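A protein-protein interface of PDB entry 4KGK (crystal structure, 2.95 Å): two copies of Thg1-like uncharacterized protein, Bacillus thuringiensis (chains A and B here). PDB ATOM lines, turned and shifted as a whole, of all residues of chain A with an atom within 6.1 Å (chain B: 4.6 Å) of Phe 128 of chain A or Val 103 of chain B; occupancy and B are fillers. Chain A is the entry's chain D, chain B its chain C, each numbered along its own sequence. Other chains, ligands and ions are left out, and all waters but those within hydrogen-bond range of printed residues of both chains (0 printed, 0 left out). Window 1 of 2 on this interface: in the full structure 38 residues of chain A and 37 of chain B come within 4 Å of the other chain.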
ATOM      1  N   ILE A  29      32.463  15.819  11.299  1.00  0.00           N
ATOM      2  CA  ILE A  29      31.350  16.567  11.862  1.00  0.00           C
ATOM      3  C   ILE A  29      30.106  15.691  11.914  1.00  0.00           C
ATOM      4  O   ILE A  29      29.481  15.433  10.888  1.00  0.00           O
ATOM      5  CB  ILE A  29      31.037  17.816  11.017  1.00  0.00           C
ATOM      6  CG1 ILE A  29      32.314  18.613  10.745  1.00  0.00           C
ATOM      7  CG2 ILE A  29      29.999  18.682  11.706  1.00  0.00           C
ATOM      8  CD1 ILE A  29      32.088  19.852   9.911  1.00  0.00           C
ATOM      9  N   ASP A  30      29.748  15.236  13.108  1.00  0.00           N
ATOM     10  CA  ASP A  30      28.588  14.366  13.268  1.00  0.00           C
ATOM     11  C   ASP A  30      27.421  15.099  13.921  1.00  0.00           C
ATOM     12  O   ASP A  30      27.616  15.949  14.789  1.00  0.00           O
ATOM     13  CB  ASP A  30      28.955  13.126  14.083  1.00  0.00           C
ATOM     14  CG  ASP A  30      27.810  12.143  14.193  1.00  0.00           C
ATOM     15  OD1 ASP A  30      27.013  12.264  15.148  1.00  0.00           O
ATOM     16  OD2 ASP A  30      27.708  11.249  13.324  1.00  0.00           O
ATOM     17  N   GLY A  31      26.207  14.764  13.494  1.00  0.00           N
ATOM     18  CA  GLY A  31      25.009  15.389  14.021  1.00  0.00           C
ATOM     19  C   GLY A  31      24.643  14.883  15.402  1.00  0.00           C
ATOM     20  O   GLY A  31      24.654  13.679  15.654  1.00  0.00           O
ATOM     21  N   ALA A  32      24.317  15.810  16.298  1.00  0.00           N
ATOM     22  CA  ALA A  32      23.980  15.461  17.672  1.00  0.00           C
ATOM     23  C   ALA A  32      22.496  15.148  17.823  1.00  0.00           C
ATOM     24  O   ALA A  32      21.643  15.965  17.472  1.00  0.00           O
ATOM     25  CB  ALA A  32      24.385  16.582  18.617  1.00  0.00           C
ATOM     26  N   PHE A  34      20.500  12.953  16.236  1.00  0.00           N
ATOM     27  CA  PHE A  34      19.795  12.926  14.957  1.00  0.00           C
ATOM     28  C   PHE A  34      18.740  11.825  14.910  1.00  0.00           C
ATOM     29  O   PHE A  34      17.853  11.841  14.057  1.00  0.00           O
ATOM     30  CB  PHE A  34      20.782  12.770  13.798  1.00  0.00           C
ATOM     31  CG  PHE A  34      20.954  14.017  12.981  1.00  0.00           C
ATOM     32  CD1 PHE A  34      21.542  15.143  13.528  1.00  0.00           C
ATOM     33  CD2 PHE A  34      20.530  14.060  11.662  1.00  0.00           C
ATOM     34  CE1 PHE A  34      21.704  16.293  12.778  1.00  0.00           C
ATOM     35  CE2 PHE A  34      20.689  15.206  10.906  1.00  0.00           C
ATOM     36  CZ  PHE A  34      21.277  16.325  11.464  1.00  0.00           C
ATOM     37  N   PHE A  53      22.558  17.871   3.408  1.00  0.00           N
ATOM     38  CA  PHE A  53      23.940  17.572   3.762  1.00  0.00           C
ATOM     39  C   PHE A  53      24.877  17.931   2.616  1.00  0.00           C
ATOM     40  O   PHE A  53      25.938  18.521   2.830  1.00  0.00           O
ATOM     41  CB  PHE A  53      24.100  16.091   4.108  1.00  0.00           C
ATOM     42  CG  PHE A  53      23.868  15.773   5.559  1.00  0.00           C
ATOM     43  CD1 PHE A  53      24.840  16.051   6.505  1.00  0.00           C
ATOM     44  CD2 PHE A  53      22.689  15.178   5.973  1.00  0.00           C
ATOM     45  CE1 PHE A  53      24.636  15.754   7.838  1.00  0.00           C
ATOM     46  CE2 PHE A  53      22.480  14.878   7.307  1.00  0.00           C
ATOM     47  CZ  PHE A  53      23.454  15.167   8.240  1.00  0.00           C
ATOM     48  N   THR A  56      25.568  21.409   2.392  1.00  0.00           N
ATOM     49  CA  THR A  56      26.424  21.807   3.502  1.00  0.00           C
ATOM     50  C   THR A  56      27.877  21.447   3.204  1.00  0.00           C
ATOM     51  O   THR A  56      28.788  22.231   3.473  1.00  0.00           O
ATOM     52  CB  THR A  56      25.986  21.134   4.819  1.00  0.00           C
ATOM     53  OG1 THR A  56      24.657  21.553   5.152  1.00  0.00           O
ATOM     54  CG2 THR A  56      26.924  21.511   5.951  1.00  0.00           C
ATOM     55  N   ASP A  75      24.803  10.743   9.079  1.00  0.00           N
ATOM     56  CA  ASP A  75      24.675  12.054   9.702  1.00  0.00           C
ATOM     57  C   ASP A  75      26.032  12.721   9.900  1.00  0.00           C
ATOM     58  O   ASP A  75      26.126  13.772  10.530  1.00  0.00           O
ATOM     59  CB  ASP A  75      23.964  11.933  11.051  1.00  0.00           C
ATOM     60  CG  ASP A  75      24.778  11.156  12.073  1.00  0.00           C
ATOM     61  OD1 ASP A  75      25.391  10.135  11.697  1.00  0.00           O
ATOM     62  OD2 ASP A  75      24.807  11.571  13.251  1.00  0.00           O
ATOM     63  N   ILE A  77      30.027  14.065   8.465  1.00  0.00           N
ATOM     64  CA  ILE A  77      30.747  14.658   7.347  1.00  0.00           C
ATOM     65  C   ILE A  77      32.245  14.693   7.635  1.00  0.00           C
ATOM     66  O   ILE A  77      32.685  15.335   8.588  1.00  0.00           O
ATOM     67  CB  ILE A  77      30.267  16.096   7.067  1.00  0.00           C
ATOM     68  CG1 ILE A  77      28.814  16.097   6.589  1.00  0.00           C
ATOM     69  CG2 ILE A  77      31.158  16.762   6.034  1.00  0.00           C
ATOM     70  CD1 ILE A  77      28.265  17.482   6.305  1.00  0.00           C
ATOM     71  N   ALA A 105      32.153  22.707  12.820  1.00  0.00           N
ATOM     72  CA  ALA A 105      30.855  22.296  13.338  1.00  0.00           C
ATOM     73  C   ALA A 105      29.861  23.448  13.263  1.00  0.00           C
ATOM     74  O   ALA A 105      28.659  23.232  13.107  1.00  0.00           O
ATOM     75  CB  ALA A 105      30.988  21.802  14.767  1.00  0.00           C
ATOM     76  N   SER A 106      30.369  24.672  13.368  1.00  0.00           N
ATOM     77  CA  SER A 106      29.530  25.863  13.289  1.00  0.00           C
ATOM     78  C   SER A 106      29.083  26.140  11.859  1.00  0.00           C
ATOM     79  O   SER A 106      27.909  26.421  11.613  1.00  0.00           O
ATOM     80  CB  SER A 106      30.267  27.081  13.849  1.00  0.00           C
ATOM     81  OG  SER A 106      29.546  28.274  13.588  1.00  0.00           O
ATOM     82  N   ALA A 108      28.917  23.990   9.467  1.00  0.00           N
ATOM     83  CA  ALA A 108      28.026  22.894   9.117  1.00  0.00           C
ATOM     84  C   ALA A 108      26.631  23.121   9.681  1.00  0.00           C
ATOM     85  O   ALA A 108      25.637  22.732   9.077  1.00  0.00           O
ATOM     86  CB  ALA A 108      28.589  21.572   9.614  1.00  0.00           C
ATOM     87  N   THR A 109      26.565  23.765  10.841  1.00  0.00           N
ATOM     88  CA  THR A 109      25.292  23.999  11.508  1.00  0.00           C
ATOM     89  C   THR A 109      24.466  25.077  10.808  1.00  0.00           C
ATOM     90  O   THR A 109      23.283  24.880  10.533  1.00  0.00           O
ATOM     91  CB  THR A 109      25.502  24.395  12.981  1.00  0.00           C
ATOM     92  OG1 THR A 109      26.265  23.379  13.645  1.00  0.00           O
ATOM     93  CG2 THR A 109      24.166  24.558  13.685  1.00  0.00           C
ATOM     94  N   PHE A 112      23.258  23.997   7.217  1.00  0.00           N
ATOM     95  CA  PHE A 112      22.304  22.895   7.264  1.00  0.00           C
ATOM     96  C   PHE A 112      20.922  23.382   7.676  1.00  0.00           C
ATOM     97  O   PHE A 112      19.917  23.000   7.076  1.00  0.00           O
ATOM     98  CB  PHE A 112      22.786  21.813   8.230  1.00  0.00           C
ATOM     99  CG  PHE A 112      21.937  20.577   8.235  1.00  0.00           C
ATOM    100  CD1 PHE A 112      22.189  19.548   7.346  1.00  0.00           C
ATOM    101  CD2 PHE A 112      20.897  20.435   9.140  1.00  0.00           C
ATOM    102  CE1 PHE A 112      21.416  18.405   7.352  1.00  0.00           C
ATOM    103  CE2 PHE A 112      20.119  19.295   9.150  1.00  0.00           C
ATOM    104  CZ  PHE A 112      20.379  18.280   8.255  1.00  0.00           C
ATOM    105  N   ASN A 113      20.875  24.222   8.703  1.00  0.00           N
ATOM    106  CA  ASN A 113      19.611  24.778   9.170  1.00  0.00           C
ATOM    107  C   ASN A 113      18.960  25.683   8.131  1.00  0.00           C
ATOM    108  O   ASN A 113      17.742  25.678   7.977  1.00  0.00           O
ATOM    109  CB  ASN A 113      19.802  25.534  10.486  1.00  0.00           C
ATOM    110  CG  ASN A 113      20.159  24.617  11.640  1.00  0.00           C
ATOM    111  OD1 ASN A 113      19.284  24.107  12.340  1.00  0.00           O
ATOM    112  ND2 ASN A 113      21.453  24.406  11.848  1.00  0.00           N
ATOM    113  N   ALA A 126      18.913  21.755  14.326  1.00  0.00           N
ATOM    114  CA  ALA A 126      19.875  20.663  14.304  1.00  0.00           C
ATOM    115  C   ALA A 126      21.264  21.176  14.665  1.00  0.00           C
ATOM    116  O   ALA A 126      21.679  22.243  14.208  1.00  0.00           O
ATOM    117  CB  ALA A 126      19.891  20.004  12.937  1.00  0.00           C
ATOM    118  N   THR A 127      21.980  20.414  15.486  1.00  0.00           N
ATOM    119  CA  THR A 127      23.319  20.802  15.917  1.00  0.00           C
ATOM    120  C   THR A 127      24.352  19.732  15.570  1.00  0.00           C
ATOM    121  O   THR A 127      24.004  18.583  15.298  1.00  0.00           O
ATOM    122  CB  THR A 127      23.363  21.100  17.431  1.00  0.00           C
ATOM    123  OG1 THR A 127      22.810  19.994  18.155  1.00  0.00           O
ATOM    124  CG2 THR A 127      22.562  22.354  17.750  1.00  0.00           C
ATOM    125  N   PHE A 128      25.623  20.120  15.579  1.00  0.00           N
ATOM    126  CA  PHE A 128      26.705  19.218  15.195  1.00  0.00           C
ATOM    127  C   PHE A 128      27.874  19.280  16.171  1.00  0.00           C
ATOM    128  O   PHE A 128      28.085  20.288  16.840  1.00  0.00           O
ATOM    129  CB  PHE A 128      27.214  19.567  13.794  1.00  0.00           C
ATOM    130  CG  PHE A 128      26.225  19.287  12.699  1.00  0.00           C
ATOM    131  CD1 PHE A 128      25.365  20.275  12.255  1.00  0.00           C
ATOM    132  CD2 PHE A 128      26.166  18.037  12.107  1.00  0.00           C
ATOM    133  CE1 PHE A 128      24.459  20.021  11.247  1.00  0.00           C
ATOM    134  CE2 PHE A 128      25.261  17.776  11.097  1.00  0.00           C
ATOM    135  CZ  PHE A 128      24.405  18.770  10.668  1.00  0.00           C
ATOM    136  N   ASP A 129      28.635  18.194  16.240  1.00  0.00           N
ATOM    137  CA  ASP A 129      29.888  18.197  16.984  1.00  0.00           C
ATOM    138  C   ASP A 129      31.030  17.906  16.024  1.00  0.00           C
ATOM    139  O   ASP A 129      30.898  17.073  15.127  1.00  0.00           O
ATOM    140  CB  ASP A 129      29.863  17.177  18.127  1.00  0.00           C
ATOM    141  CG  ASP A 129      30.066  15.753  17.650  1.00  0.00           C
ATOM    142  OD1 ASP A 129      29.071  15.111  17.253  1.00  0.00           O
ATOM    143  OD2 ASP A 129      31.221  15.275  17.680  1.00  0.00           O
ATOM    144  N   GLY A 130      32.145  18.605  16.202  1.00  0.00           N
ATOM    145  CA  GLY A 130      33.283  18.450  15.316  1.00  0.00           C
ATOM    146  C   GLY A 130      34.551  18.053  16.043  1.00  0.00           C
ATOM    147  O   GLY A 130      34.795  18.487  17.168  1.00  0.00           O
ATOM    148  N   TRP B  92      29.560  17.182  31.396  1.00  0.00           N
ATOM    149  CA  TRP B  92      29.042  17.387  30.050  1.00  0.00           C
ATOM    150  C   TRP B  92      30.012  16.789  29.037  1.00  0.00           C
ATOM    151  O   TRP B  92      31.143  17.262  28.902  1.00  0.00           O
ATOM    152  CB  TRP B  92      28.853  18.880  29.776  1.00  0.00           C
ATOM    153  CG  TRP B  92      28.090  19.166  28.524  1.00  0.00           C
ATOM    154  CD1 TRP B  92      27.118  18.389  27.963  1.00  0.00           C
ATOM    155  CD2 TRP B  92      28.241  20.303  27.666  1.00  0.00           C
ATOM    156  NE1 TRP B  92      26.649  18.977  26.813  1.00  0.00           N
ATOM    157  CE2 TRP B  92      27.322  20.152  26.608  1.00  0.00           C
ATOM    158  CE3 TRP B  92      29.062  21.434  27.692  1.00  0.00           C
ATOM    159  CZ2 TRP B  92      27.203  21.090  25.583  1.00  0.00           C
ATOM    160  CZ3 TRP B  92      28.941  22.365  26.673  1.00  0.00           C
ATOM    161  CH2 TRP B  92      28.019  22.186  25.634  1.00  0.00           C
ATOM    162  N   PHE B  93      29.568  15.743  28.344  1.00  0.00           N
ATOM    163  CA  PHE B  93      30.398  15.024  27.378  1.00  0.00           C
ATOM    164  C   PHE B  93      31.676  14.474  28.014  1.00  0.00           C
ATOM    165  O   PHE B  93      32.692  14.321  27.335  1.00  0.00           O
ATOM    166  CB  PHE B  93      30.758  15.918  26.185  1.00  0.00           C
ATOM    167  CG  PHE B  93      29.571  16.399  25.401  1.00  0.00           C
ATOM    168  CD1 PHE B  93      28.491  15.565  25.164  1.00  0.00           C
ATOM    169  CD2 PHE B  93      29.534  17.691  24.903  1.00  0.00           C
ATOM    170  CE1 PHE B  93      27.398  16.010  24.441  1.00  0.00           C
ATOM    171  CE2 PHE B  93      28.444  18.142  24.182  1.00  0.00           C
ATOM    172  CZ  PHE B  93      27.375  17.301  23.951  1.00  0.00           C
ATOM    173  N   LYS B  99      34.517  18.309  21.935  1.00  0.00           N
ATOM    174  CA  LYS B  99      33.067  18.177  21.861  1.00  0.00           C
ATOM    175  C   LYS B  99      32.361  19.350  22.536  1.00  0.00           C
ATOM    176  O   LYS B  99      31.303  19.789  22.089  1.00  0.00           O
ATOM    177  CB  LYS B  99      32.610  16.850  22.475  1.00  0.00           C
ATOM    178  CG  LYS B  99      31.404  16.232  21.784  1.00  0.00           C
ATOM    179  CD  LYS B  99      31.147  14.819  22.279  1.00  0.00           C
ATOM    180  CE  LYS B  99      30.224  14.056  21.338  1.00  0.00           C
ATOM    181  NZ  LYS B  99      28.894  14.711  21.194  1.00  0.00           N
ATOM    182  N   ILE B 100      32.952  19.858  23.612  1.00  0.00           N
ATOM    183  CA  ILE B 100      32.384  21.000  24.316  1.00  0.00           C
ATOM    184  C   ILE B 100      32.515  22.267  23.476  1.00  0.00           C
ATOM    185  O   ILE B 100      31.562  23.032  23.336  1.00  0.00           O
ATOM    186  CB  ILE B 100      33.056  21.214  25.687  1.00  0.00           C
ATOM    187  CG1 ILE B 100      32.782  20.023  26.604  1.00  0.00           C
ATOM    188  CG2 ILE B 100      32.557  22.495  26.336  1.00  0.00           C
ATOM    189  CD1 ILE B 100      33.400  20.161  27.974  1.00  0.00           C
ATOM    190  N   ALA B 101      33.697  22.472  22.905  1.00  0.00           N
ATOM    191  CA  ALA B 101      33.969  23.663  22.107  1.00  0.00           C
ATOM    192  C   ALA B 101      33.134  23.703  20.829  1.00  0.00           C
ATOM    193  O   ALA B 101      32.705  24.770  20.395  1.00  0.00           O
ATOM    194  CB  ALA B 101      35.454  23.751  21.777  1.00  0.00           C
ATOM    195  N   SER B 102      32.905  22.537  20.235  1.00  0.00           N
ATOM    196  CA  SER B 102      32.196  22.459  18.963  1.00  0.00           C
ATOM    197  C   SER B 102      30.677  22.555  19.115  1.00  0.00           C
ATOM    198  O   SER B 102      30.028  23.337  18.417  1.00  0.00           O
ATOM    199  CB  SER B 102      32.581  21.183  18.207  1.00  0.00           C
ATOM    200  OG  SER B 102      32.325  20.027  18.983  1.00  0.00           O
ATOM    201  N   VAL B 103      30.112  21.758  20.019  1.00  0.00           N
ATOM    202  CA  VAL B 103      28.666  21.753  20.238  1.00  0.00           C
ATOM    203  C   VAL B 103      28.163  23.114  20.714  1.00  0.00           C
ATOM    204  O   VAL B 103      27.145  23.612  20.231  1.00  0.00           O
ATOM    205  CB  VAL B 103      28.240  20.656  21.239  1.00  0.00           C
ATOM    206  CG1 VAL B 103      26.790  20.838  21.656  1.00  0.00           C
ATOM    207  CG2 VAL B 103      28.447  19.281  20.634  1.00  0.00           C
ATOM    208  N   SER B 104      28.887  23.714  21.654  1.00  0.00           N
ATOM    209  CA  SER B 104      28.542  25.039  22.152  1.00  0.00           C
ATOM    210  C   SER B 104      28.529  26.043  21.011  1.00  0.00           C
ATOM    211  O   SER B 104      27.606  26.847  20.888  1.00  0.00           O
ATOM    212  CB  SER B 104      29.528  25.484  23.231  1.00  0.00           C
ATOM    213  OG  SER B 104      29.500  24.602  24.338  1.00  0.00           O
ATOM    214  N   ALA B 105      29.561  25.985  20.176  1.00  0.00           N
ATOM    215  CA  ALA B 105      29.642  26.838  19.000  1.00  0.00           C
ATOM    216  C   ALA B 105      28.489  26.529  18.054  1.00  0.00           C
ATOM    217  O   ALA B 105      27.895  27.432  17.470  1.00  0.00           O
ATOM    218  CB  ALA B 105      30.972  26.644  18.296  1.00  0.00           C
ATOM    219  N   SER B 106      28.173  25.245  17.917  1.00  0.00           N
ATOM    220  CA  SER B 106      27.088  24.806  17.048  1.00  0.00           C
ATOM    221  C   SER B 106      25.735  25.293  17.553  1.00  0.00           C
ATOM    222  O   SER B 106      24.902  25.750  16.772  1.00  0.00           O
ATOM    223  CB  SER B 106      27.085  23.284  16.929  1.00  0.00           C
ATOM    224  OG  SER B 106      25.989  22.835  16.150  1.00  0.00           O
ATOM    225  N   MET B 107      25.519  25.187  18.860  1.00  0.00           N
ATOM    226  CA  MET B 107      24.278  25.658  19.465  1.00  0.00           C
ATOM    227  C   MET B 107      24.156  27.173  19.344  1.00  0.00           C
ATOM    228  O   MET B 107      23.093  27.695  19.012  1.00  0.00           O
ATOM    229  CB  MET B 107      24.195  25.235  20.933  1.00  0.00           C
ATOM    230  CG  MET B 107      23.997  23.742  21.137  1.00  0.00           C
ATOM    231  SD  MET B 107      23.827  23.302  22.876  1.00  0.00           S
ATOM    232  CE  MET B 107      25.361  23.955  23.520  1.00  0.00           C
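Of the 20 printed residues of chain A, 6 touch a printed residue of chain B.
Printed residues of chain A that touch a printed residue of chain B: Ala 105, Thr 109, Thr 127, Phe 128, Asp 129 and Gly 130.
Hydrophobic or aromatic side chains of chain B within 4 Å of the printed part of chain A: Val 103 and Met 107.
Along chain B the printed residues that touch a printed residue of chain A span positions 99 to 107.
Among the printed residues, 11 pairs touch across the chains.
Among the printed residues, Asp or Glu carboxylates within 4 Å of a Lys or Arg side-chain nitrogen of the other chain: Asp 129 of chain A with Lys 99 of chain B (3.97 Å).
Phe 128 of chain A touches just these residues of chain B: Ser 102, Val 103 and Ser 106.
Of the printed residues of chain A, Val 103 of chain B touches Phe 128 and Asp 129.
Of the printed residues of chain B, Ala 105 of chain A touches Ser 102.
Printed residues of chain B within 4 Å of Thr 127 of chain A: Ser 106 and Met 107.
Of the printed residues of chain B, Asp 129 of chain A touches Lys 99 (3.9 Å), Ser 102 (3.6 Å) and Val 103 (3.6 Å).
Printed residues of chain A within 4 Å of Met 107 of chain B: Thr 127.
Of the printed residues of chain B, Thr 109 of chain A touches Ser 106.
Ile 100 of chain B touches none of the printed residues of chain A.
Trp 92 of chain B touches none of the printed residues of chain A.
The nearest printed residue of chain B that does not touch Phe 128 of chain A is Met 107 of chain B (5.9 Å).
The nearest printed residue of chain B that does not touch Ala 105 of chain A is Ser 106 of chain B (4.1 Å).
The side-chain hydroxyl (OG) of Ser 102 of chain B sits at hydrogen-bond distance from the backbone carbonyl oxygen (O) of Lys 99 of chain B, 3.3 Å away.
The backbone carbonyl oxygen (O) of Asp 30 of chain A lies within hydrogen-bond range of the backbone NH (N) of Asp 129 of chain A.
N of Ala 32 of chain A lies within hydrogen-bond range of O of Thr 127 of chain A.
O of Ala 105 of chain A is in hydrogen-bond range of OG1 of Thr 109 of chain A (2.5 Å).
Positions printed for both chains: 105 and 106.
Of the 11 pairs that touch across the chains among the printed residues, none has its exchanged pair printed and touching as well.
The side-chain carboxylate of Asp 129 of chain A is in salt-bridge range of the side-chain amino group of Lys 99 of chain B.
N of Gly 130 of chain A is in hydrogen-bond range of OG of Ser 102 of chain B (3.1 Å).
OG of Ser 106 of chain B lies within hydrogen-bond range of OG1 of Thr 109 of chain A, 2.6 Å away.
OG of Ser 106 of chain B is in hydrogen-bond range of N of Phe 128 of chain A.
Ala 105 of chain A touches Ser 102 of chain B.
Ser 106 of chain B touches Thr 127 of chain A (OG to CA, 3.4 Å).
Thr 127 of chain A touches Met 107 of chain B (CG2 to CG, 3.9 Å).
O of Ser 102 of chain B touches O of Phe 128 of chain A (3.9 Å).
O of Phe 128 of chain A touches CA of Val 103 of chain B, at 3.7 Å.
CA of Asp 129 of chain A touches OG of Ser 102 of chain B, 3.6 Å away.
Val 103 of chain B touches Asp 129 of chain A (CG2 to CB, 3.6 Å).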
